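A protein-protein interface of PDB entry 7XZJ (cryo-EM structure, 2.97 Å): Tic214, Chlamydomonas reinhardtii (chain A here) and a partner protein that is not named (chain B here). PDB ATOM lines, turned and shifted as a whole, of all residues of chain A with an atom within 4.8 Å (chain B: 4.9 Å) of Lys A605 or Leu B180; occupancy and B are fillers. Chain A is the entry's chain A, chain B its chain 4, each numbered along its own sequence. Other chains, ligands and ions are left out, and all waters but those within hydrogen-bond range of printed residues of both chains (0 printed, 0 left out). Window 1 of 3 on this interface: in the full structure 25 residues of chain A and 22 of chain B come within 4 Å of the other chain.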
ATOM      1  N   ILE A 599      14.467   1.365 -17.607  1.00  0.00           N
ATOM      2  CA  ILE A 599      13.859   2.676 -17.792  1.00  0.00           C
ATOM      3  C   ILE A 599      13.560   3.264 -16.422  1.00  0.00           C
ATOM      4  O   ILE A 599      12.880   2.633 -15.603  1.00  0.00           O
ATOM      5  CB  ILE A 599      12.584   2.583 -18.644  1.00  0.00           C
ATOM      6  CG1 ILE A 599      12.876   1.850 -19.954  1.00  0.00           C
ATOM      7  CG2 ILE A 599      12.031   3.969 -18.919  1.00  0.00           C
ATOM      8  CD1 ILE A 599      11.667   1.695 -20.847  1.00  0.00           C
ATOM      9  N   TYR A 600      14.116   4.442 -16.137  1.00  0.00           N
ATOM     10  CA  TYR A 600      13.952   5.028 -14.782  1.00  0.00           C
ATOM     11  C   TYR A 600      13.009   6.232 -14.855  1.00  0.00           C
ATOM     12  O   TYR A 600      12.949   6.876 -15.913  1.00  0.00           O
ATOM     13  CB  TYR A 600      15.318   5.413 -14.208  1.00  0.00           C
ATOM     14  CG  TYR A 600      16.261   4.256 -13.994  1.00  0.00           C
ATOM     15  CD1 TYR A 600      17.082   3.806 -15.012  1.00  0.00           C
ATOM     16  CD2 TYR A 600      16.334   3.613 -12.772  1.00  0.00           C
ATOM     17  CE1 TYR A 600      17.949   2.742 -14.823  1.00  0.00           C
ATOM     18  CE2 TYR A 600      17.195   2.549 -12.564  1.00  0.00           C
ATOM     19  CZ  TYR A 600      18.007   2.111 -13.595  1.00  0.00           C
ATOM     20  OH  TYR A 600      18.859   1.063 -13.400  1.00  0.00           O
ATOM     21  N   SER A 601      12.292   6.516 -13.765  1.00  0.00           N
ATOM     22  CA  SER A 601      11.417   7.714 -13.744  1.00  0.00           C
ATOM     23  C   SER A 601      12.283   8.962 -13.587  1.00  0.00           C
ATOM     24  O   SER A 601      13.103   8.995 -12.652  1.00  0.00           O
ATOM     25  CB  SER A 601      10.414   7.626 -12.635  1.00  0.00           C
ATOM     26  OG  SER A 601       9.673   8.832 -12.531  1.00  0.00           O
ATOM     27  N   LYS A 602      12.096   9.950 -14.463  1.00  0.00           N
ATOM     28  CA  LYS A 602      12.852  11.222 -14.341  1.00  0.00           C
ATOM     29  C   LYS A 602      12.451  11.917 -13.037  1.00  0.00           C
ATOM     30  O   LYS A 602      13.355  12.392 -12.323  1.00  0.00           O
ATOM     31  CB  LYS A 602      12.556  12.110 -15.553  1.00  0.00           C
ATOM     32  CG  LYS A 602      13.306  13.435 -15.596  1.00  0.00           C
ATOM     33  CD  LYS A 602      12.966  14.264 -16.814  1.00  0.00           C
ATOM     34  CE  LYS A 602      13.672  15.602 -16.838  1.00  0.00           C
ATOM     35  NZ  LYS A 602      13.288  16.402 -18.024  1.00  0.00           N
ATOM     36  N   ARG A 603      11.150  11.950 -12.730  1.00  0.00           N
ATOM     37  CA  ARG A 603      10.669  12.664 -11.517  1.00  0.00           C
ATOM     38  C   ARG A 603      11.225  11.996 -10.257  1.00  0.00           C
ATOM     39  O   ARG A 603      11.734  12.720  -9.378  1.00  0.00           O
ATOM     40  CB  ARG A 603       9.137  12.660 -11.489  1.00  0.00           C
ATOM     41  CG  ARG A 603       8.535  13.093 -10.160  1.00  0.00           C
ATOM     42  CD  ARG A 603       7.030  12.918 -10.135  1.00  0.00           C
ATOM     43  NE  ARG A 603       6.364  13.775 -11.106  1.00  0.00           N
ATOM     44  CZ  ARG A 603       5.049  13.838 -11.274  1.00  0.00           C
ATOM     45  NH1 ARG A 603       4.252  13.088 -10.532  1.00  0.00           N
ATOM     46  NH2 ARG A 603       4.536  14.649 -12.181  1.00  0.00           N
ATOM     47  N   TRP A 604      11.167  10.662 -10.194  1.00  0.00           N
ATOM     48  CA  TRP A 604      11.643   9.940  -8.985  1.00  0.00           C
ATOM     49  C   TRP A 604      13.147  10.170  -8.834  1.00  0.00           C
ATOM     50  O   TRP A 604      13.590  10.445  -7.704  1.00  0.00           O
ATOM     51  CB  TRP A 604      11.302   8.448  -9.061  1.00  0.00           C
ATOM     52  CG  TRP A 604       9.833   8.156  -9.065  1.00  0.00           C
ATOM     53  CD1 TRP A 604       8.813   9.036  -8.849  1.00  0.00           C
ATOM     54  CD2 TRP A 604       9.214   6.878  -9.298  1.00  0.00           C
ATOM     55  NE1 TRP A 604       7.605   8.398  -8.934  1.00  0.00           N
ATOM     56  CE2 TRP A 604       7.820   7.073  -9.209  1.00  0.00           C
ATOM     57  CE3 TRP A 604       9.698   5.595  -9.574  1.00  0.00           C
ATOM     58  CZ2 TRP A 604       6.912   6.031  -9.386  1.00  0.00           C
ATOM     59  CZ3 TRP A 604       8.800   4.567  -9.750  1.00  0.00           C
ATOM     60  CH2 TRP A 604       7.426   4.785  -9.656  1.00  0.00           C
ATOM     61  N   LYS A 605      13.885  10.116  -9.946  1.00  0.00           N
ATOM     62  CA  LYS A 605      15.360  10.276  -9.886  1.00  0.00           C
ATOM     63  C   LYS A 605      15.671  11.669  -9.339  1.00  0.00           C
ATOM     64  O   LYS A 605      16.565  11.778  -8.484  1.00  0.00           O
ATOM     65  CB  LYS A 605      15.967  10.127 -11.284  1.00  0.00           C
ATOM     66  CG  LYS A 605      17.486  10.041 -11.322  1.00  0.00           C
ATOM     67  CD  LYS A 605      18.061  10.106 -12.717  1.00  0.00           C
ATOM     68  CE  LYS A 605      19.531   9.750 -12.751  1.00  0.00           C
ATOM     69  NZ  LYS A 605      20.166  10.138 -14.031  1.00  0.00           N
ATOM     70  N   SER A 606      14.929  12.679  -9.796  1.00  0.00           N
ATOM     71  CA  SER A 606      15.196  14.071  -9.355  1.00  0.00           C
ATOM     72  C   SER A 606      14.973  14.183  -7.844  1.00  0.00           C
ATOM     73  O   SER A 606      15.810  14.814  -7.176  1.00  0.00           O
ATOM     74  CB  SER A 606      14.329  15.043 -10.108  1.00  0.00           C
ATOM     75  OG  SER A 606      14.531  14.919 -11.508  1.00  0.00           O
ATOM     76  N   ILE A 607      13.897  13.578  -7.331  1.00  0.00           N
ATOM     77  CA  ILE A 607      13.580  13.690  -5.875  1.00  0.00           C
ATOM     78  C   ILE A 607      14.701  13.030  -5.062  1.00  0.00           C
ATOM     79  O   ILE A 607      15.170  13.653  -4.089  1.00  0.00           O
ATOM     80  CB  ILE A 607      12.211  13.047  -5.574  1.00  0.00           C
ATOM     81  CG1 ILE A 607      11.067  13.794  -6.264  1.00  0.00           C
ATOM     82  CG2 ILE A 607      11.981  12.934  -4.076  1.00  0.00           C
ATOM     83  CD1 ILE A 607      10.865  15.202  -5.760  1.00  0.00           C
ATOM     84  N   PHE A 608      15.133  11.833  -5.469  1.00  0.00           N
ATOM     85  CA  PHE A 608      16.187  11.101  -4.718  1.00  0.00           C
ATOM     86  C   PHE A 608      17.518  11.855  -4.805  1.00  0.00           C
ATOM     87  O   PHE A 608      18.244  11.912  -3.798  1.00  0.00           O
ATOM     88  CB  PHE A 608      16.255   9.638  -5.164  1.00  0.00           C
ATOM     89  CG  PHE A 608      14.997   8.860  -4.871  1.00  0.00           C
ATOM     90  CD1 PHE A 608      14.422   8.898  -3.611  1.00  0.00           C
ATOM     91  CD2 PHE A 608      14.386   8.094  -5.849  1.00  0.00           C
ATOM     92  CE1 PHE A 608      13.262   8.191  -3.337  1.00  0.00           C
ATOM     93  CE2 PHE A 608      13.225   7.388  -5.577  1.00  0.00           C
ATOM     94  CZ  PHE A 608      12.666   7.437  -4.321  1.00  0.00           C
ATOM     95  N   SER A 609      17.838  12.395  -5.983  1.00  0.00           N
ATOM     96  CA  SER A 609      19.089  13.181  -6.151  1.00  0.00           C
ATOM     97  C   SER A 609      19.027  14.438  -5.282  1.00  0.00           C
ATOM     98  O   SER A 609      20.064  14.797  -4.694  1.00  0.00           O
ATOM     99  CB  SER A 609      19.316  13.527  -7.597  1.00  0.00           C
ATOM    100  OG  SER A 609      19.365  12.352  -8.393  1.00  0.00           O
ATOM    101  N   ILE A 647      14.341   4.126  -7.792  1.00  0.00           N
ATOM    102  CA  ILE A 647      14.144   4.981  -9.003  1.00  0.00           C
ATOM    103  C   ILE A 647      13.474   4.183 -10.128  1.00  0.00           C
ATOM    104  O   ILE A 647      12.618   4.764 -10.824  1.00  0.00           O
ATOM    105  CB  ILE A 647      15.487   5.589  -9.450  1.00  0.00           C
ATOM    106  CG1 ILE A 647      16.210   6.266  -8.284  1.00  0.00           C
ATOM    107  CG2 ILE A 647      15.294   6.539 -10.619  1.00  0.00           C
ATOM    108  CD1 ILE A 647      17.421   7.066  -8.693  1.00  0.00           C
ATOM    109  N   LYS B 178      21.499   6.692 -18.252  1.00  0.00           N
ATOM    110  CA  LYS B 178      20.374   5.718 -18.272  1.00  0.00           C
ATOM    111  C   LYS B 178      19.164   6.356 -18.959  1.00  0.00           C
ATOM    112  O   LYS B 178      18.978   7.578 -18.812  1.00  0.00           O
ATOM    113  CB  LYS B 178      20.010   5.333 -16.835  1.00  0.00           C
ATOM    114  CG  LYS B 178      21.159   4.790 -15.994  1.00  0.00           C
ATOM    115  CD  LYS B 178      20.899   4.842 -14.504  1.00  0.00           C
ATOM    116  CE  LYS B 178      20.698   6.249 -13.985  1.00  0.00           C
ATOM    117  NZ  LYS B 178      21.897   7.091 -14.205  1.00  0.00           N
ATOM    118  N   VAL B 179      18.374   5.558 -19.682  1.00  0.00           N
ATOM    119  CA  VAL B 179      17.143   6.085 -20.342  1.00  0.00           C
ATOM    120  C   VAL B 179      16.182   6.558 -19.247  1.00  0.00           C
ATOM    121  O   VAL B 179      16.068   5.859 -18.221  1.00  0.00           O
ATOM    122  CB  VAL B 179      16.492   5.014 -21.239  1.00  0.00           C
ATOM    123  CG1 VAL B 179      15.235   5.526 -21.926  1.00  0.00           C
ATOM    124  CG2 VAL B 179      17.475   4.468 -22.263  1.00  0.00           C
ATOM    125  N   LEU B 180      15.515   7.694 -19.463  1.00  0.00           N
ATOM    126  CA  LEU B 180      14.582   8.251 -18.447  1.00  0.00           C
ATOM    127  C   LEU B 180      13.189   8.366 -19.068  1.00  0.00           C
ATOM    128  O   LEU B 180      13.113   8.543 -20.291  1.00  0.00           O
ATOM    129  CB  LEU B 180      15.084   9.627 -18.000  1.00  0.00           C
ATOM    130  CG  LEU B 180      16.309   9.626 -17.089  1.00  0.00           C
ATOM    131  CD1 LEU B 180      16.697  11.047 -16.709  1.00  0.00           C
ATOM    132  CD2 LEU B 180      16.053   8.796 -15.841  1.00  0.00           C
ATOM    133  N   TYR B 181      12.137   8.236 -18.259  1.00  0.00           N
ATOM    134  CA  TYR B 181      10.756   8.420 -18.775  1.00  0.00           C
ATOM    135  C   TYR B 181      10.166   9.698 -18.177  1.00  0.00           C
ATOM    136  O   TYR B 181      10.163   9.827 -16.938  1.00  0.00           O
ATOM    137  CB  TYR B 181       9.876   7.217 -18.424  1.00  0.00           C
ATOM    138  CG  TYR B 181       8.397   7.465 -18.577  1.00  0.00           C
ATOM    139  CD1 TYR B 181       7.843   7.752 -19.813  1.00  0.00           C
ATOM    140  CD2 TYR B 181       7.548   7.416 -17.484  1.00  0.00           C
ATOM    141  CE1 TYR B 181       6.486   7.986 -19.960  1.00  0.00           C
ATOM    142  CE2 TYR B 181       6.189   7.646 -17.613  1.00  0.00           C
ATOM    143  CZ  TYR B 181       5.656   7.932 -18.857  1.00  0.00           C
ATOM    144  OH  TYR B 181       4.317   8.161 -18.992  1.00  0.00           O
ATOM    145  N   ASN B 182       9.685  10.611 -19.027  1.00  0.00           N
ATOM    146  CA  ASN B 182       9.010  11.820 -18.493  1.00  0.00           C
ATOM    147  C   ASN B 182       7.504  11.573 -18.570  1.00  0.00           C
ATOM    148  O   ASN B 182       7.001  11.377 -19.692  1.00  0.00           O
ATOM    149  CB  ASN B 182       9.411  13.084 -19.256  1.00  0.00           C
ATOM    150  CG  ASN B 182       9.275  14.337 -18.419  1.00  0.00           C
ATOM    151  OD1 ASN B 182       9.349  14.279 -17.194  1.00  0.00           O
ATOM    152  ND2 ASN B 182       9.084  15.473 -19.069  1.00  0.00           N
ATOM    153  N   LEU B 187       6.530  10.144 -23.048  1.00  0.00           N
ATOM    154  CA  LEU B 187       7.480   9.535 -24.017  1.00  0.00           C
ATOM    155  C   LEU B 187       8.807   9.301 -23.289  1.00  0.00           C
ATOM    156  O   LEU B 187       9.062  10.011 -22.297  1.00  0.00           O
ATOM    157  CB  LEU B 187       7.686  10.496 -25.192  1.00  0.00           C
ATOM    158  CG  LEU B 187       6.474  10.742 -26.088  1.00  0.00           C
ATOM    159  CD1 LEU B 187       6.766  11.834 -27.102  1.00  0.00           C
ATOM    160  CD2 LEU B 187       6.050   9.463 -26.794  1.00  0.00           C
ATOM    161  N   LEU B 188       9.617   8.352 -23.768  1.00  0.00           N
ATOM    162  CA  LEU B 188      10.951   8.122 -23.153  1.00  0.00           C
ATOM    163  C   LEU B 188      11.897   9.247 -23.569  1.00  0.00           C
ATOM    164  O   LEU B 188      11.856   9.642 -24.743  1.00  0.00           O
ATOM    165  CB  LEU B 188      11.495   6.780 -23.642  1.00  0.00           C
ATOM    166  CG  LEU B 188      10.677   5.555 -23.244  1.00  0.00           C
ATOM    167  CD1 LEU B 188      11.361   4.281 -23.709  1.00  0.00           C
ATOM    168  CD2 LEU B 188      10.474   5.525 -21.740  1.00  0.00           C
ATOM    169  N   GLU B 189      12.725   9.735 -22.647  1.00  0.00           N
ATOM    170  CA  GLU B 189      13.745  10.741 -23.035  1.00  0.00           C
ATOM    171  C   GLU B 189      15.070   9.990 -23.153  1.00  0.00           C
ATOM    172  O   GLU B 189      15.548   9.479 -22.123  1.00  0.00           O
ATOM    173  CB  GLU B 189      13.833  11.847 -21.986  1.00  0.00           C
ATOM    174  CG  GLU B 189      12.485  12.452 -21.640  1.00  0.00           C
ATOM    175  CD  GLU B 189      11.778  13.128 -22.803  1.00  0.00           C
ATOM    176  OE1 GLU B 189      12.455  13.833 -23.577  1.00  0.00           O
ATOM    177  OE2 GLU B 189      10.555  12.937 -22.937  1.00  0.00           O
ATOM    178  N   TYR B 236      25.564   4.407  -7.096  1.00  0.00           N
ATOM    179  CA  TYR B 236      24.349   3.546  -7.040  1.00  0.00           C
ATOM    180  C   TYR B 236      24.578   2.134  -6.488  1.00  0.00           C
ATOM    181  O   TYR B 236      23.717   1.674  -5.713  1.00  0.00           O
ATOM    182  CB  TYR B 236      23.694   3.467  -8.421  1.00  0.00           C
ATOM    183  CG  TYR B 236      22.893   4.686  -8.797  1.00  0.00           C
ATOM    184  CD1 TYR B 236      23.456   5.712  -9.537  1.00  0.00           C
ATOM    185  CD2 TYR B 236      21.573   4.821  -8.402  1.00  0.00           C
ATOM    186  CE1 TYR B 236      22.727   6.837  -9.883  1.00  0.00           C
ATOM    187  CE2 TYR B 236      20.831   5.939  -8.737  1.00  0.00           C
ATOM    188  CZ  TYR B 236      21.409   6.952  -9.482  1.00  0.00           C
ATOM    189  OH  TYR B 236      20.685   8.058  -9.817  1.00  0.00           O
ATOM    190  N   ASP B 263      24.140  13.105  -9.144  1.00  0.00           N
ATOM    191  CA  ASP B 263      23.816  13.221 -10.590  1.00  0.00           C
ATOM    192  C   ASP B 263      22.771  14.323 -10.788  1.00  0.00           C
ATOM    193  O   ASP B 263      21.820  14.384  -9.986  1.00  0.00           O
ATOM    194  CB  ASP B 263      23.343  11.880 -11.157  1.00  0.00           C
ATOM    195  CG  ASP B 263      22.332  11.174 -10.272  1.00  0.00           C
ATOM    196  OD1 ASP B 263      22.758  10.384  -9.409  1.00  0.00           O
ATOM    197  OD2 ASP B 263      21.125  11.426 -10.448  1.00  0.00           O
ATOM    198  N   ASP B 265      19.998  15.638 -13.544  1.00  0.00           N
ATOM    199  CA  ASP B 265      19.350  15.194 -14.810  1.00  0.00           C
ATOM    200  C   ASP B 265      20.060  13.917 -15.269  1.00  0.00           C
ATOM    201  O   ASP B 265      20.262  13.024 -14.423  1.00  0.00           O
ATOM    202  CB  ASP B 265      19.371  16.289 -15.880  1.00  0.00           C
ATOM    203  CG  ASP B 265      18.707  17.582 -15.441  1.00  0.00           C
ATOM    204  OD1 ASP B 265      18.038  17.568 -14.389  1.00  0.00           O
ATOM    205  OD2 ASP B 265      18.868  18.592 -16.151  1.00  0.00           O
ATOM    206  N   GLU B 266      20.420  13.830 -16.552  1.00  0.00           N
ATOM    207  CA  GLU B 266      21.219  12.669 -17.029  1.00  0.00           C
ATOM    208  C   GLU B 266      22.651  13.160 -17.261  1.00  0.00           C
ATOM    209  O   GLU B 266      23.476  12.377 -17.769  1.00  0.00           O
ATOM    210  CB  GLU B 266      20.582  12.049 -18.274  1.00  0.00           C
ATOM    211  CG  GLU B 266      20.950  10.589 -18.473  1.00  0.00           C
ATOM    212  CD  GLU B 266      20.900   9.754 -17.205  1.00  0.00           C
ATOM    213  OE1 GLU B 266      19.786   9.452 -16.742  1.00  0.00           O
ATOM    214  OE2 GLU B 266      21.977   9.412 -16.679  1.00  0.00           O
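The side-chain hydroxyl (OG) of Ser A609 lies within hydrogen-bond range of the side-chain carboxylate (OD2) of Asp B263 (2.9 Å).
OD2 of Asp B263 lies within salt-bridge range of NZ of Lys A605 (3.9 Å).
The backbone carbonyl oxygen (O) of Val B179 sits at hydrogen-bond distance from the backbone NH (N) of Tyr A600 (3.2 Å).
The backbone NH of Lys A602 sits at hydrogen-bond distance from the backbone carbonyl oxygen of Tyr B181 (3.1 Å).
O of Tyr A600 sits at hydrogen-bond distance from N of Tyr B181.
The backbone carbonyl oxygen of Asp B265 is in hydrogen-bond range of the side-chain amino group of Lys A605 (2.9 Å).
The side-chain carboxylate (OE1) of Glu B266 is in salt-bridge range of the side-chain amino group (NZ) of Lys A605 (2.8 Å).
O of Lys A602 sits at hydrogen-bond distance from OG of Ser A606, at 2.9 Å.
N of Ser A601 lies within hydrogen-bond range of O of Ile A647, 3.4 Å away.
N of Asn B182 is in hydrogen-bond range of O of Leu B187, at 3.4 Å.
O of Lys A605 is in hydrogen-bond range of OG of Ser A609 (2.9 Å).
The side-chain carboxylate of Glu B266 is in salt-bridge range of the side-chain amino group of Lys B178 (3.4 Å).
O of Leu B180 is in hydrogen-bond range of N of Glu B189.
Val B179 touches Ile A599 (O to CA, 3.9 Å).
Tyr B181 touches Ile A599.
Ile A599 touches Leu B188.
CE1 of Tyr A600 touches CD of Lys B178, 3.6 Å away.
O of Tyr A600 touches CA of Leu B180, 3.3 Å away.
OD1 of Asn B182 touches CD of Lys A602, 3.6 Å away.
Lys B178 touches Lys A605 (NZ to NZ, 3.5 Å).
Lys A605 touches Leu B180 (CD to CD2, 3.9 Å).
Lys A605 touches Tyr B236.
CD1 of Ile A647 touches CE2 of Tyr B236 (3.6 Å).
Lys A605 touches just these residues of chain B: Lys B178 (3.5 Å), Leu B180 (3.9 Å), Tyr B236 (3.6 Å), Asp B263 (3.3 Å), Asp B265 (2.9 Å) and Glu B266 (2.8 Å).
Of chain A, only Tyr A600 (3.3 Å) and Lys A605 (3.9 Å) come within 4 Å of Leu B180.
Of the printed residues of chain A, Leu B188 touches Ile A599 (3.6 Å).
Of the printed residues of chain B, Ser A609 touches Asp B263 (2.9 Å).
Of the printed residues of chain A, Lys B178 touches Tyr A600 (3.6 Å) and Lys A605 (3.5 Å).
Of the printed residues of chain B, Lys A602 touches Tyr B181 (3.1 Å) and Asn B182 (3.6 Å).
The nearest residue of chain A that does not touch Leu B180 is Lys A602 (4.3 Å).
The nearest printed residue of chain A that does not touch Asp B265 is Ser A606 (5.3 Å).
Of the 12 printed residues of chain A, 6 touch a printed residue of chain B.
Hydrophobic or aromatic side chains of chain A that line the printed part of chain B: Ile A599, Tyr A600 and Ile A647.
Among the printed residues, 17 pairs touch across the chains.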
